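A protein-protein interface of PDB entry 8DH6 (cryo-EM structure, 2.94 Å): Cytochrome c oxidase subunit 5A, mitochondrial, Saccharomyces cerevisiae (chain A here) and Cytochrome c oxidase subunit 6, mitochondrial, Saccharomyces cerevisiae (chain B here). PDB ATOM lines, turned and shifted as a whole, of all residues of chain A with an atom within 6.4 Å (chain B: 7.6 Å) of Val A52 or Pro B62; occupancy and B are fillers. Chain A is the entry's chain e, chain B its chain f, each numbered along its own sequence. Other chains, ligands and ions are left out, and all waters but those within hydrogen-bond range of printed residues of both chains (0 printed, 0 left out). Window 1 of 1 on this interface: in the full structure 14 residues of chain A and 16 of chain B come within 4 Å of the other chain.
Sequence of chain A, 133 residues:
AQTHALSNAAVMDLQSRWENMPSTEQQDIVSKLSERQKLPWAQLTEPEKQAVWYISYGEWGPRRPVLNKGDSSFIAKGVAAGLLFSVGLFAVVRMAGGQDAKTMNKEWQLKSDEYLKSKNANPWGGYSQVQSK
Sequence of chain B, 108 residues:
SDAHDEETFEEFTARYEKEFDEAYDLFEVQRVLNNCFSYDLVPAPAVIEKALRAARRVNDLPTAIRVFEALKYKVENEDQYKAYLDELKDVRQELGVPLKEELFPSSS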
ATOM      1  N   LEU A  14     -17.366  18.408  -9.637  1.00  0.00           N
ATOM      2  CA  LEU A  14     -18.451  18.860  -8.775  1.00  0.00           C
ATOM      3  C   LEU A  14     -18.894  20.274  -9.125  1.00  0.00           C
ATOM      4  O   LEU A  14     -20.029  20.660  -8.826  1.00  0.00           O
ATOM      5  CB  LEU A  14     -18.025  18.781  -7.310  1.00  0.00           C
ATOM      6  CG  LEU A  14     -19.145  18.929  -6.281  1.00  0.00           C
ATOM      7  CD1 LEU A  14     -20.142  17.797  -6.435  1.00  0.00           C
ATOM      8  CD2 LEU A  14     -18.587  18.960  -4.875  1.00  0.00           C
ATOM      9  N   LEU A  33     -17.294  14.110   3.043  1.00  0.00           N
ATOM     10  CA  LEU A  33     -16.115  14.964   2.975  1.00  0.00           C
ATOM     11  C   LEU A  33     -15.750  15.526   4.342  1.00  0.00           C
ATOM     12  O   LEU A  33     -14.564  15.678   4.647  1.00  0.00           O
ATOM     13  CB  LEU A  33     -16.343  16.090   1.968  1.00  0.00           C
ATOM     14  CG  LEU A  33     -16.197  15.665   0.505  1.00  0.00           C
ATOM     15  CD1 LEU A  33     -16.632  16.780  -0.422  1.00  0.00           C
ATOM     16  CD2 LEU A  33     -14.770  15.240   0.207  1.00  0.00           C
ATOM     17  N   SER A  34     -16.742  15.829   5.182  1.00  0.00           N
ATOM     18  CA  SER A  34     -16.445  16.291   6.533  1.00  0.00           C
ATOM     19  C   SER A  34     -15.825  15.187   7.376  1.00  0.00           C
ATOM     20  O   SER A  34     -14.972  15.464   8.226  1.00  0.00           O
ATOM     21  CB  SER A  34     -17.711  16.820   7.201  1.00  0.00           C
ATOM     22  OG  SER A  34     -18.390  17.728   6.353  1.00  0.00           O
ATOM     23  N   GLN A  37     -12.268  15.104   6.295  1.00  0.00           N
ATOM     24  CA  GLN A  37     -11.473  16.242   6.750  1.00  0.00           C
ATOM     25  C   GLN A  37     -10.635  15.907   7.976  1.00  0.00           C
ATOM     26  O   GLN A  37      -9.519  16.416   8.120  1.00  0.00           O
ATOM     27  CB  GLN A  37     -12.377  17.432   7.069  1.00  0.00           C
ATOM     28  CG  GLN A  37     -13.043  18.070   5.874  1.00  0.00           C
ATOM     29  CD  GLN A  37     -12.058  18.791   4.996  1.00  0.00           C
ATOM     30  OE1 GLN A  37     -11.141  19.442   5.488  1.00  0.00           O
ATOM     31  NE2 GLN A  37     -12.235  18.681   3.687  1.00  0.00           N
ATOM     32  N   TRP A  41      -4.385  16.434   6.309  1.00  0.00           N
ATOM     33  CA  TRP A  41      -4.778  17.023   5.036  1.00  0.00           C
ATOM     34  C   TRP A  41      -3.863  16.629   3.887  1.00  0.00           C
ATOM     35  O   TRP A  41      -4.215  16.879   2.730  1.00  0.00           O
ATOM     36  CB  TRP A  41      -4.834  18.544   5.157  1.00  0.00           C
ATOM     37  CG  TRP A  41      -6.009  19.020   5.943  1.00  0.00           C
ATOM     38  CD1 TRP A  41      -7.141  18.317   6.228  1.00  0.00           C
ATOM     39  CD2 TRP A  41      -6.174  20.307   6.542  1.00  0.00           C
ATOM     40  NE1 TRP A  41      -8.000  19.086   6.972  1.00  0.00           N
ATOM     41  CE2 TRP A  41      -7.429  20.314   7.178  1.00  0.00           C
ATOM     42  CE3 TRP A  41      -5.380  21.455   6.603  1.00  0.00           C
ATOM     43  CZ2 TRP A  41      -7.909  21.422   7.865  1.00  0.00           C
ATOM     44  CZ3 TRP A  41      -5.858  22.552   7.285  1.00  0.00           C
ATOM     45  CH2 TRP A  41      -7.110  22.530   7.907  1.00  0.00           C
ATOM     46  N   LEU A  44      -5.686  13.818   1.688  1.00  0.00           N
ATOM     47  CA  LEU A  44      -6.803  14.122   0.804  1.00  0.00           C
ATOM     48  C   LEU A  44      -6.308  14.301  -0.623  1.00  0.00           C
ATOM     49  O   LEU A  44      -5.339  15.023  -0.869  1.00  0.00           O
ATOM     50  CB  LEU A  44      -7.533  15.380   1.270  1.00  0.00           C
ATOM     51  CG  LEU A  44      -8.605  15.208   2.347  1.00  0.00           C
ATOM     52  CD1 LEU A  44      -7.971  15.050   3.717  1.00  0.00           C
ATOM     53  CD2 LEU A  44      -9.574  16.378   2.326  1.00  0.00           C
ATOM     54  N   PRO A  47      -8.940  16.038  -6.231  1.00  0.00           N
ATOM     55  CA  PRO A  47     -10.378  16.237  -6.460  1.00  0.00           C
ATOM     56  C   PRO A  47     -11.164  16.444  -5.182  1.00  0.00           C
ATOM     57  O   PRO A  47     -12.122  17.224  -5.184  1.00  0.00           O
ATOM     58  CB  PRO A  47     -10.799  14.949  -7.177  1.00  0.00           C
ATOM     59  CG  PRO A  47      -9.562  14.489  -7.842  1.00  0.00           C
ATOM     60  CD  PRO A  47      -8.473  14.793  -6.865  1.00  0.00           C
ATOM     61  N   GLU A  48     -10.791  15.777  -4.089  1.00  0.00           N
ATOM     62  CA  GLU A  48     -11.480  15.995  -2.823  1.00  0.00           C
ATOM     63  C   GLU A  48     -11.272  17.415  -2.315  1.00  0.00           C
ATOM     64  O   GLU A  48     -12.219  18.056  -1.844  1.00  0.00           O
ATOM     65  CB  GLU A  48     -11.003  14.981  -1.788  1.00  0.00           C
ATOM     66  CG  GLU A  48     -11.856  13.736  -1.711  1.00  0.00           C
ATOM     67  CD  GLU A  48     -11.405  12.804  -0.614  1.00  0.00           C
ATOM     68  OE1 GLU A  48     -10.208  12.451  -0.596  1.00  0.00           O
ATOM     69  OE2 GLU A  48     -12.241  12.427   0.233  1.00  0.00           O
ATOM     70  N   LYS A  49     -10.041  17.923  -2.399  1.00  0.00           N
ATOM     71  CA  LYS A  49      -9.780  19.297  -1.982  1.00  0.00           C
ATOM     72  C   LYS A  49     -10.572  20.285  -2.827  1.00  0.00           C
ATOM     73  O   LYS A  49     -11.166  21.231  -2.295  1.00  0.00           O
ATOM     74  CB  LYS A  49      -8.284  19.596  -2.071  1.00  0.00           C
ATOM     75  CG  LYS A  49      -7.436  18.825  -1.079  1.00  0.00           C
ATOM     76  CD  LYS A  49      -5.960  19.112  -1.274  1.00  0.00           C
ATOM     77  CE  LYS A  49      -5.108  18.237  -0.372  1.00  0.00           C
ATOM     78  NZ  LYS A  49      -3.672  18.271  -0.760  1.00  0.00           N
ATOM     79  N   GLN A  50     -10.600  20.076  -4.146  1.00  0.00           N
ATOM     80  CA  GLN A  50     -11.364  20.961  -5.016  1.00  0.00           C
ATOM     81  C   GLN A  50     -12.851  20.901  -4.695  1.00  0.00           C
ATOM     82  O   GLN A  50     -13.529  21.933  -4.667  1.00  0.00           O
ATOM     83  CB  GLN A  50     -11.118  20.601  -6.479  1.00  0.00           C
ATOM     84  CG  GLN A  50      -9.687  20.790  -6.931  1.00  0.00           C
ATOM     85  CD  GLN A  50      -9.492  20.428  -8.386  1.00  0.00           C
ATOM     86  OE1 GLN A  50     -10.406  19.931  -9.040  1.00  0.00           O
ATOM     87  NE2 GLN A  50      -8.296  20.676  -8.902  1.00  0.00           N
ATOM     88  N   ALA A  51     -13.376  19.698  -4.455  1.00  0.00           N
ATOM     89  CA  ALA A  51     -14.789  19.555  -4.131  1.00  0.00           C
ATOM     90  C   ALA A  51     -15.133  20.262  -2.830  1.00  0.00           C
ATOM     91  O   ALA A  51     -16.156  20.949  -2.743  1.00  0.00           O
ATOM     92  CB  ALA A  51     -15.158  18.076  -4.047  1.00  0.00           C
ATOM     93  N   VAL A  52     -14.289  20.108  -1.809  1.00  0.00           N
ATOM     94  CA  VAL A  52     -14.550  20.758  -0.529  1.00  0.00           C
ATOM     95  C   VAL A  52     -14.493  22.273  -0.677  1.00  0.00           C
ATOM     96  O   VAL A  52     -15.349  22.998  -0.147  1.00  0.00           O
ATOM     97  CB  VAL A  52     -13.561  20.251   0.534  1.00  0.00           C
ATOM     98  CG1 VAL A  52     -13.724  21.033   1.809  1.00  0.00           C
ATOM     99  CG2 VAL A  52     -13.785  18.775   0.794  1.00  0.00           C
ATOM    100  N   TRP A  53     -13.491  22.780  -1.402  1.00  0.00           N
ATOM    101  CA  TRP A  53     -13.404  24.220  -1.601  1.00  0.00           C
ATOM    102  C   TRP A  53     -14.600  24.753  -2.373  1.00  0.00           C
ATOM    103  O   TRP A  53     -15.106  25.830  -2.051  1.00  0.00           O
ATOM    104  CB  TRP A  53     -12.111  24.597  -2.322  1.00  0.00           C
ATOM    105  CG  TRP A  53     -11.918  26.083  -2.383  1.00  0.00           C
ATOM    106  CD1 TRP A  53     -11.233  26.854  -1.492  1.00  0.00           C
ATOM    107  CD2 TRP A  53     -12.439  26.979  -3.371  1.00  0.00           C
ATOM    108  NE1 TRP A  53     -11.287  28.173  -1.869  1.00  0.00           N
ATOM    109  CE2 TRP A  53     -12.022  28.276  -3.019  1.00  0.00           C
ATOM    110  CE3 TRP A  53     -13.213  26.810  -4.523  1.00  0.00           C
ATOM    111  CZ2 TRP A  53     -12.353  29.395  -3.775  1.00  0.00           C
ATOM    112  CZ3 TRP A  53     -13.540  27.922  -5.271  1.00  0.00           C
ATOM    113  CH2 TRP A  53     -13.110  29.197  -4.895  1.00  0.00           C
ATOM    114  N   TYR A  54     -15.058  24.035  -3.400  1.00  0.00           N
ATOM    115  CA  TYR A  54     -16.224  24.492  -4.143  1.00  0.00           C
ATOM    116  C   TYR A  54     -17.493  24.439  -3.305  1.00  0.00           C
ATOM    117  O   TYR A  54     -18.355  25.310  -3.441  1.00  0.00           O
ATOM    118  CB  TYR A  54     -16.414  23.668  -5.413  1.00  0.00           C
ATOM    119  CG  TYR A  54     -17.589  24.129  -6.239  1.00  0.00           C
ATOM    120  CD1 TYR A  54     -17.521  25.297  -6.983  1.00  0.00           C
ATOM    121  CD2 TYR A  54     -18.772  23.407  -6.263  1.00  0.00           C
ATOM    122  CE1 TYR A  54     -18.593  25.727  -7.734  1.00  0.00           C
ATOM    123  CE2 TYR A  54     -19.849  23.831  -7.010  1.00  0.00           C
ATOM    124  CZ  TYR A  54     -19.755  24.991  -7.744  1.00  0.00           C
ATOM    125  OH  TYR A  54     -20.827  25.416  -8.491  1.00  0.00           O
ATOM    126  N   ILE A  55     -17.635  23.423  -2.454  1.00  0.00           N
ATOM    127  CA  ILE A  55     -18.797  23.360  -1.575  1.00  0.00           C
ATOM    128  C   ILE A  55     -18.800  24.540  -0.613  1.00  0.00           C
ATOM    129  O   ILE A  55     -19.845  25.151  -0.363  1.00  0.00           O
ATOM    130  CB  ILE A  55     -18.830  22.017  -0.828  1.00  0.00           C
ATOM    131  CG1 ILE A  55     -19.155  20.883  -1.797  1.00  0.00           C
ATOM    132  CG2 ILE A  55     -19.841  22.055   0.300  1.00  0.00           C
ATOM    133  CD1 ILE A  55     -18.971  19.513  -1.207  1.00  0.00           C
ATOM    134  N   SER A  56     -17.635  24.888  -0.067  1.00  0.00           N
ATOM    135  CA  SER A  56     -17.589  25.959   0.923  1.00  0.00           C
ATOM    136  C   SER A  56     -17.699  27.338   0.276  1.00  0.00           C
ATOM    137  O   SER A  56     -18.595  28.120   0.608  1.00  0.00           O
ATOM    138  CB  SER A  56     -16.308  25.852   1.750  1.00  0.00           C
ATOM    139  OG  SER A  56     -16.301  24.650   2.496  1.00  0.00           O
ATOM    140  N   TYR A  57     -16.798  27.652  -0.650  1.00  0.00           N
ATOM    141  CA  TYR A  57     -16.664  28.992  -1.211  1.00  0.00           C
ATOM    142  C   TYR A  57     -16.956  29.031  -2.708  1.00  0.00           C
ATOM    143  O   TYR A  57     -16.445  29.889  -3.429  1.00  0.00           O
ATOM    144  CB  TYR A  57     -15.270  29.544  -0.945  1.00  0.00           C
ATOM    145  CG  TYR A  57     -14.903  29.594   0.514  1.00  0.00           C
ATOM    146  CD1 TYR A  57     -15.460  30.543   1.349  1.00  0.00           C
ATOM    147  CD2 TYR A  57     -13.993  28.698   1.053  1.00  0.00           C
ATOM    148  CE1 TYR A  57     -15.130  30.597   2.678  1.00  0.00           C
ATOM    149  CE2 TYR A  57     -13.656  28.747   2.386  1.00  0.00           C
ATOM    150  CZ  TYR A  57     -14.228  29.701   3.193  1.00  0.00           C
ATOM    151  OH  TYR A  57     -13.902  29.765   4.526  1.00  0.00           O
ATOM    152  N   LEU B  26     -16.193  26.003  13.947  1.00  0.00           N
ATOM    153  CA  LEU B  26     -15.967  26.601  12.635  1.00  0.00           C
ATOM    154  C   LEU B  26     -16.563  27.998  12.533  1.00  0.00           C
ATOM    155  O   LEU B  26     -15.938  28.894  11.953  1.00  0.00           O
ATOM    156  CB  LEU B  26     -16.541  25.701  11.544  1.00  0.00           C
ATOM    157  CG  LEU B  26     -16.387  26.220  10.117  1.00  0.00           C
ATOM    158  CD1 LEU B  26     -14.925  26.483   9.820  1.00  0.00           C
ATOM    159  CD2 LEU B  26     -16.970  25.230   9.128  1.00  0.00           C
ATOM    160  N   GLN B  30     -14.221  31.229  11.654  1.00  0.00           N
ATOM    161  CA  GLN B  30     -14.493  32.079  10.501  1.00  0.00           C
ATOM    162  C   GLN B  30     -14.809  33.508  10.924  1.00  0.00           C
ATOM    163  O   GLN B  30     -14.376  34.459  10.268  1.00  0.00           O
ATOM    164  CB  GLN B  30     -15.634  31.487   9.678  1.00  0.00           C
ATOM    165  CG  GLN B  30     -15.285  30.154   9.048  1.00  0.00           C
ATOM    166  CD  GLN B  30     -16.131  29.836   7.839  1.00  0.00           C
ATOM    167  OE1 GLN B  30     -17.300  30.206   7.774  1.00  0.00           O
ATOM    168  NE2 GLN B  30     -15.546  29.139   6.875  1.00  0.00           N
ATOM    169  N   LEU B  33     -11.527  35.168  11.999  1.00  0.00           N
ATOM    170  CA  LEU B  33     -10.726  35.463  10.818  1.00  0.00           C
ATOM    171  C   LEU B  33     -11.305  36.642  10.040  1.00  0.00           C
ATOM    172  O   LEU B  33     -10.558  37.508   9.563  1.00  0.00           O
ATOM    173  CB  LEU B  33     -10.634  34.212   9.947  1.00  0.00           C
ATOM    174  CG  LEU B  33      -9.868  34.261   8.632  1.00  0.00           C
ATOM    175  CD1 LEU B  33      -8.390  34.389   8.912  1.00  0.00           C
ATOM    176  CD2 LEU B  33     -10.150  33.001   7.843  1.00  0.00           C
ATOM    177  N   ALA B  55      -8.013  26.425  12.034  1.00  0.00           N
ATOM    178  CA  ALA B  55      -8.643  25.715  10.927  1.00  0.00           C
ATOM    179  C   ALA B  55      -8.361  24.220  10.985  1.00  0.00           C
ATOM    180  O   ALA B  55      -9.246  23.410  10.689  1.00  0.00           O
ATOM    181  CB  ALA B  55      -8.171  26.292   9.595  1.00  0.00           C
ATOM    182  N   ASN B  59     -11.048  21.087  11.828  1.00  0.00           N
ATOM    183  CA  ASN B  59     -11.085  20.195  10.670  1.00  0.00           C
ATOM    184  C   ASN B  59     -11.857  20.821   9.507  1.00  0.00           C
ATOM    185  O   ASN B  59     -12.894  20.321   9.068  1.00  0.00           O
ATOM    186  CB  ASN B  59     -11.669  18.832  11.053  1.00  0.00           C
ATOM    187  CG  ASN B  59     -11.128  18.317  12.370  1.00  0.00           C
ATOM    188  OD1 ASN B  59      -9.925  18.366  12.621  1.00  0.00           O
ATOM    189  ND2 ASN B  59     -12.016  17.821  13.220  1.00  0.00           N
ATOM    190  N   ASP B  60     -11.327  21.938   9.011  1.00  0.00           N
ATOM    191  CA  ASP B  60     -11.910  22.635   7.867  1.00  0.00           C
ATOM    192  C   ASP B  60     -10.782  23.064   6.939  1.00  0.00           C
ATOM    193  O   ASP B  60     -10.149  24.099   7.165  1.00  0.00           O
ATOM    194  CB  ASP B  60     -12.739  23.840   8.309  1.00  0.00           C
ATOM    195  CG  ASP B  60     -13.812  24.209   7.301  1.00  0.00           C
ATOM    196  OD1 ASP B  60     -14.499  23.294   6.801  1.00  0.00           O
ATOM    197  OD2 ASP B  60     -13.958  25.412   6.997  1.00  0.00           O
ATOM    198  N   LEU B  61     -10.528  22.265   5.902  1.00  0.00           N
ATOM    199  CA  LEU B  61      -9.519  22.623   4.906  1.00  0.00           C
ATOM    200  C   LEU B  61      -9.826  23.924   4.170  1.00  0.00           C
ATOM    201  O   LEU B  61      -8.924  24.772   4.054  1.00  0.00           O
ATOM    202  CB  LEU B  61      -9.337  21.457   3.932  1.00  0.00           C
ATOM    203  CG  LEU B  61      -8.317  21.605   2.803  1.00  0.00           C
ATOM    204  CD1 LEU B  61      -7.013  22.200   3.304  1.00  0.00           C
ATOM    205  CD2 LEU B  61      -8.067  20.256   2.167  1.00  0.00           C
ATOM    206  N   PRO B  62     -11.039  24.150   3.641  1.00  0.00           N
ATOM    207  CA  PRO B  62     -11.240  25.315   2.766  1.00  0.00           C
ATOM    208  C   PRO B  62     -10.985  26.653   3.433  1.00  0.00           C
ATOM    209  O   PRO B  62     -10.532  27.578   2.750  1.00  0.00           O
ATOM    210  CB  PRO B  62     -12.701  25.179   2.329  1.00  0.00           C
ATOM    211  CG  PRO B  62     -13.336  24.432   3.411  1.00  0.00           C
ATOM    212  CD  PRO B  62     -12.315  23.459   3.895  1.00  0.00           C
ATOM    213  N   THR B  63     -11.259  26.801   4.731  1.00  0.00           N
ATOM    214  CA  THR B  63     -10.961  28.071   5.384  1.00  0.00           C
ATOM    215  C   THR B  63      -9.462  28.298   5.535  1.00  0.00           C
ATOM    216  O   THR B  63      -9.019  29.451   5.522  1.00  0.00           O
ATOM    217  CB  THR B  63     -11.661  28.155   6.744  1.00  0.00           C
ATOM    218  OG1 THR B  63     -11.413  29.438   7.331  1.00  0.00           O
ATOM    219  CG2 THR B  63     -11.168  27.073   7.678  1.00  0.00           C
ATOM    220  N   ALA B  64      -8.669  27.232   5.645  1.00  0.00           N
ATOM    221  CA  ALA B  64      -7.219  27.385   5.643  1.00  0.00           C
ATOM    222  C   ALA B  64      -6.706  27.903   4.304  1.00  0.00           C
ATOM    223  O   ALA B  64      -5.788  28.729   4.277  1.00  0.00           O
ATOM    224  CB  ALA B  64      -6.547  26.059   5.992  1.00  0.00           C
ATOM    225  N   ILE B  65      -7.275  27.428   3.193  1.00  0.00           N
ATOM    226  CA  ILE B  65      -6.954  27.994   1.888  1.00  0.00           C
ATOM    227  C   ILE B  65      -7.442  29.433   1.796  1.00  0.00           C
ATOM    228  O   ILE B  65      -6.754  30.303   1.241  1.00  0.00           O
ATOM    229  CB  ILE B  65      -7.559  27.131   0.766  1.00  0.00           C
ATOM    230  CG1 ILE B  65      -7.206  25.658   0.968  1.00  0.00           C
ATOM    231  CG2 ILE B  65      -7.083  27.610  -0.588  1.00  0.00           C
ATOM    232  CD1 ILE B  65      -7.929  24.727   0.026  1.00  0.00           C
ATOM    233  N   ARG B  66      -8.635  29.704   2.325  1.00  0.00           N
ATOM    234  CA  ARG B  66      -9.187  31.050   2.311  1.00  0.00           C
ATOM    235  C   ARG B  66      -8.339  32.029   3.103  1.00  0.00           C
ATOM    236  O   ARG B  66      -8.361  33.221   2.802  1.00  0.00           O
ATOM    237  CB  ARG B  66     -10.609  31.037   2.863  1.00  0.00           C
ATOM    238  CG  ARG B  66     -11.486  32.135   2.313  1.00  0.00           C
ATOM    239  CD  ARG B  66     -11.627  32.013   0.811  1.00  0.00           C
ATOM    240  NE  ARG B  66     -12.870  32.604   0.336  1.00  0.00           N
ATOM    241  CZ  ARG B  66     -13.211  32.699  -0.940  1.00  0.00           C
ATOM    242  NH1 ARG B  66     -12.418  32.257  -1.901  1.00  0.00           N
ATOM    243  NH2 ARG B  66     -14.376  33.252  -1.261  1.00  0.00           N
ATOM    244  N   VAL B  67      -7.605  31.557   4.110  1.00  0.00           N
ATOM    245  CA  VAL B  67      -6.695  32.440   4.837  1.00  0.00           C
ATOM    246  C   VAL B  67      -5.662  33.031   3.885  1.00  0.00           C
ATOM    247  O   VAL B  67      -5.468  34.251   3.824  1.00  0.00           O
ATOM    248  CB  VAL B  67      -6.021  31.682   5.993  1.00  0.00           C
ATOM    249  CG1 VAL B  67      -4.854  32.478   6.530  1.00  0.00           C
ATOM    250  CG2 VAL B  67      -7.018  31.390   7.093  1.00  0.00           C
ATOM    251  N   PHE B  68      -5.003  32.171   3.102  1.00  0.00           N
ATOM    252  CA  PHE B  68      -4.015  32.650   2.143  1.00  0.00           C
ATOM    253  C   PHE B  68      -4.663  33.443   1.016  1.00  0.00           C
ATOM    254  O   PHE B  68      -4.074  34.410   0.524  1.00  0.00           O
ATOM    255  CB  PHE B  68      -3.221  31.478   1.572  1.00  0.00           C
ATOM    256  CG  PHE B  68      -2.234  30.890   2.534  1.00  0.00           C
ATOM    257  CD1 PHE B  68      -1.006  31.489   2.738  1.00  0.00           C
ATOM    258  CD2 PHE B  68      -2.532  29.731   3.228  1.00  0.00           C
ATOM    259  CE1 PHE B  68      -0.094  30.948   3.620  1.00  0.00           C
ATOM    260  CE2 PHE B  68      -1.625  29.185   4.111  1.00  0.00           C
ATOM    261  CZ  PHE B  68      -0.404  29.794   4.308  1.00  0.00           C
ATOM    262  N   GLU B  69      -5.865  33.047   0.591  1.00  0.00           N
ATOM    263  CA  GLU B  69      -6.557  33.809  -0.445  1.00  0.00           C
ATOM    264  C   GLU B  69      -6.868  35.227   0.024  1.00  0.00           C
ATOM    265  O   GLU B  69      -6.661  36.195  -0.718  1.00  0.00           O
ATOM    266  CB  GLU B  69      -7.834  33.082  -0.858  1.00  0.00           C
ATOM    267  CG  GLU B  69      -8.142  33.161  -2.336  1.00  0.00           C
ATOM    268  CD  GLU B  69      -9.335  32.314  -2.722  1.00  0.00           C
ATOM    269  OE1 GLU B  69      -9.628  31.335  -2.004  1.00  0.00           O
ATOM    270  OE2 GLU B  69      -9.984  32.626  -3.743  1.00  0.00           O
ATOM    271  N   VAL B  97      -1.979  22.227   3.705  1.00  0.00           N
ATOM    272  CA  VAL B  97      -2.956  23.111   3.076  1.00  0.00           C
ATOM    273  C   VAL B  97      -2.407  23.609   1.743  1.00  0.00           C
ATOM    274  O   VAL B  97      -1.278  24.112   1.682  1.00  0.00           O
ATOM    275  CB  VAL B  97      -3.338  24.273   4.009  1.00  0.00           C
ATOM    276  CG1 VAL B  97      -2.109  25.034   4.462  1.00  0.00           C
ATOM    277  CG2 VAL B  97      -4.296  25.213   3.305  1.00  0.00           C
ATOM    278  N   PRO B  98      -3.148  23.455   0.646  1.00  0.00           N
ATOM    279  CA  PRO B  98      -2.672  23.974  -0.639  1.00  0.00           C
ATOM    280  C   PRO B  98      -3.161  25.388  -0.906  1.00  0.00           C
ATOM    281  O   PRO B  98      -4.236  25.777  -0.439  1.00  0.00           O
ATOM    282  CB  PRO B  98      -3.258  22.979  -1.642  1.00  0.00           C
ATOM    283  CG  PRO B  98      -4.553  22.581  -1.015  1.00  0.00           C
ATOM    284  CD  PRO B  98      -4.363  22.636   0.487  1.00  0.00           C
ATOM    285  N   LEU B 103      -4.055  24.940  -6.250  1.00  0.00           N
ATOM    286  CA  LEU B 103      -5.068  23.893  -6.190  1.00  0.00           C
ATOM    287  C   LEU B 103      -5.910  23.846  -7.458  1.00  0.00           C
ATOM    288  O   LEU B 103      -6.231  22.759  -7.949  1.00  0.00           O
ATOM    289  CB  LEU B 103      -5.968  24.104  -4.972  1.00  0.00           C
ATOM    290  CG  LEU B 103      -7.200  23.212  -4.874  1.00  0.00           C
ATOM    291  CD1 LEU B 103      -6.787  21.767  -4.691  1.00  0.00           C
ATOM    292  CD2 LEU B 103      -8.087  23.669  -3.736  1.00  0.00           C
ATOM    293  N   PHE B 104      -6.276  25.009  -7.996  1.00  0.00           N
ATOM    294  CA  PHE B 104      -6.948  25.114  -9.283  1.00  0.00           C
ATOM    295  C   PHE B 104      -5.996  25.745 -10.291  1.00  0.00           C
ATOM    296  O   PHE B 104      -6.057  26.959 -10.521  1.00  0.00           O
ATOM    297  CB  PHE B 104      -8.224  25.952  -9.182  1.00  0.00           C
ATOM    298  CG  PHE B 104      -9.262  25.378  -8.265  1.00  0.00           C
ATOM    299  CD1 PHE B 104     -10.188  24.465  -8.734  1.00  0.00           C
ATOM    300  CD2 PHE B 104      -9.326  25.769  -6.939  1.00  0.00           C
ATOM    301  CE1 PHE B 104     -11.151  23.941  -7.896  1.00  0.00           C
ATOM    302  CE2 PHE B 104     -10.286  25.248  -6.097  1.00  0.00           C
ATOM    303  CZ  PHE B 104     -11.200  24.334  -6.578  1.00  0.00           C
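The side-chain amide nitrogen of Gln B30 sits at hydrogen-bond distance from the side-chain hydroxyl of Tyr A57.
N of Leu B61 sits at hydrogen-bond distance from OE1 of Gln A37 (2.9 Å).
The side-chain amide nitrogen (NE2) of Gln A50 sits at hydrogen-bond distance from the backbone carbonyl oxygen (O) of Leu B103 (3.1 Å).
O of Gln A37 sits at hydrogen-bond distance from NE1 of Trp A41.
O of Ala B55 is in hydrogen-bond range of N of Asp B60, at 3.1 Å.
The guanidinium group (NH1) of Arg B66 lies within salt-bridge range of the side-chain carboxylate (OE1) of Glu B69.
The backbone carbonyl oxygen of Val A52 is in hydrogen-bond range of the side-chain hydroxyl of Ser A56.
Gln A37 touches Asn B59.
Gln A37 touches Asp B60.
Asp B60 touches Trp A41 (C to CZ2, 3.4 Å).
CZ2 of Trp A41 touches N of Leu B61, 3.4 Å away.
CD1 of Leu B103 touches CB of Lys A49, 3.7 Å away.
Trp A53 touches Glu B69.
Ser A56 touches Pro B62 (OG to CG, 3.1 Å).
Pro B62 touches Tyr A57 (O to CE2, 3.4 Å).
Tyr A57 touches Thr B63 (OH to CA, 3.5 Å).
Arg B66 touches Tyr A57.
No residue of chain B comes within 4 Å of Ala A51.
Of chain B, only Pro B62 (3.5 Å) comes within 4 Å of Val A52.
Of the printed residues of chain A, Asn B59 touches Gln A37 (3.6 Å).
Of chain A, only Val A52 (3.5 Å), Ser A56 (3.1 Å) and Tyr A57 (3.4 Å) come within 4 Å of Pro B62.
Of the printed residues of chain A, Thr B63 touches Tyr A57.
Of the printed residues of chain A, Arg B66 touches Trp A53 and Tyr A57.
Printed residues of chain A that touch a printed residue of chain B: Gln A37, Trp A41, Lys A49, Gln A50, Val A52, Trp A53, Ser A56 and Tyr A57.
Hydrophobic or aromatic side chains of chain A within 4 Å of the printed part of chain B: Trp A41, Val A52, Trp A53 and Tyr A57.
Hydrophobic or aromatic side chains of chain B that line the printed part of chain A: Leu B61, Pro B62, Ala B64, Pro B98, Leu B103 and Phe B104.
Among the printed residues, no Asp or Glu carboxylate lies within 4 Å of a Lys or Arg side-chain nitrogen of the other chain.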
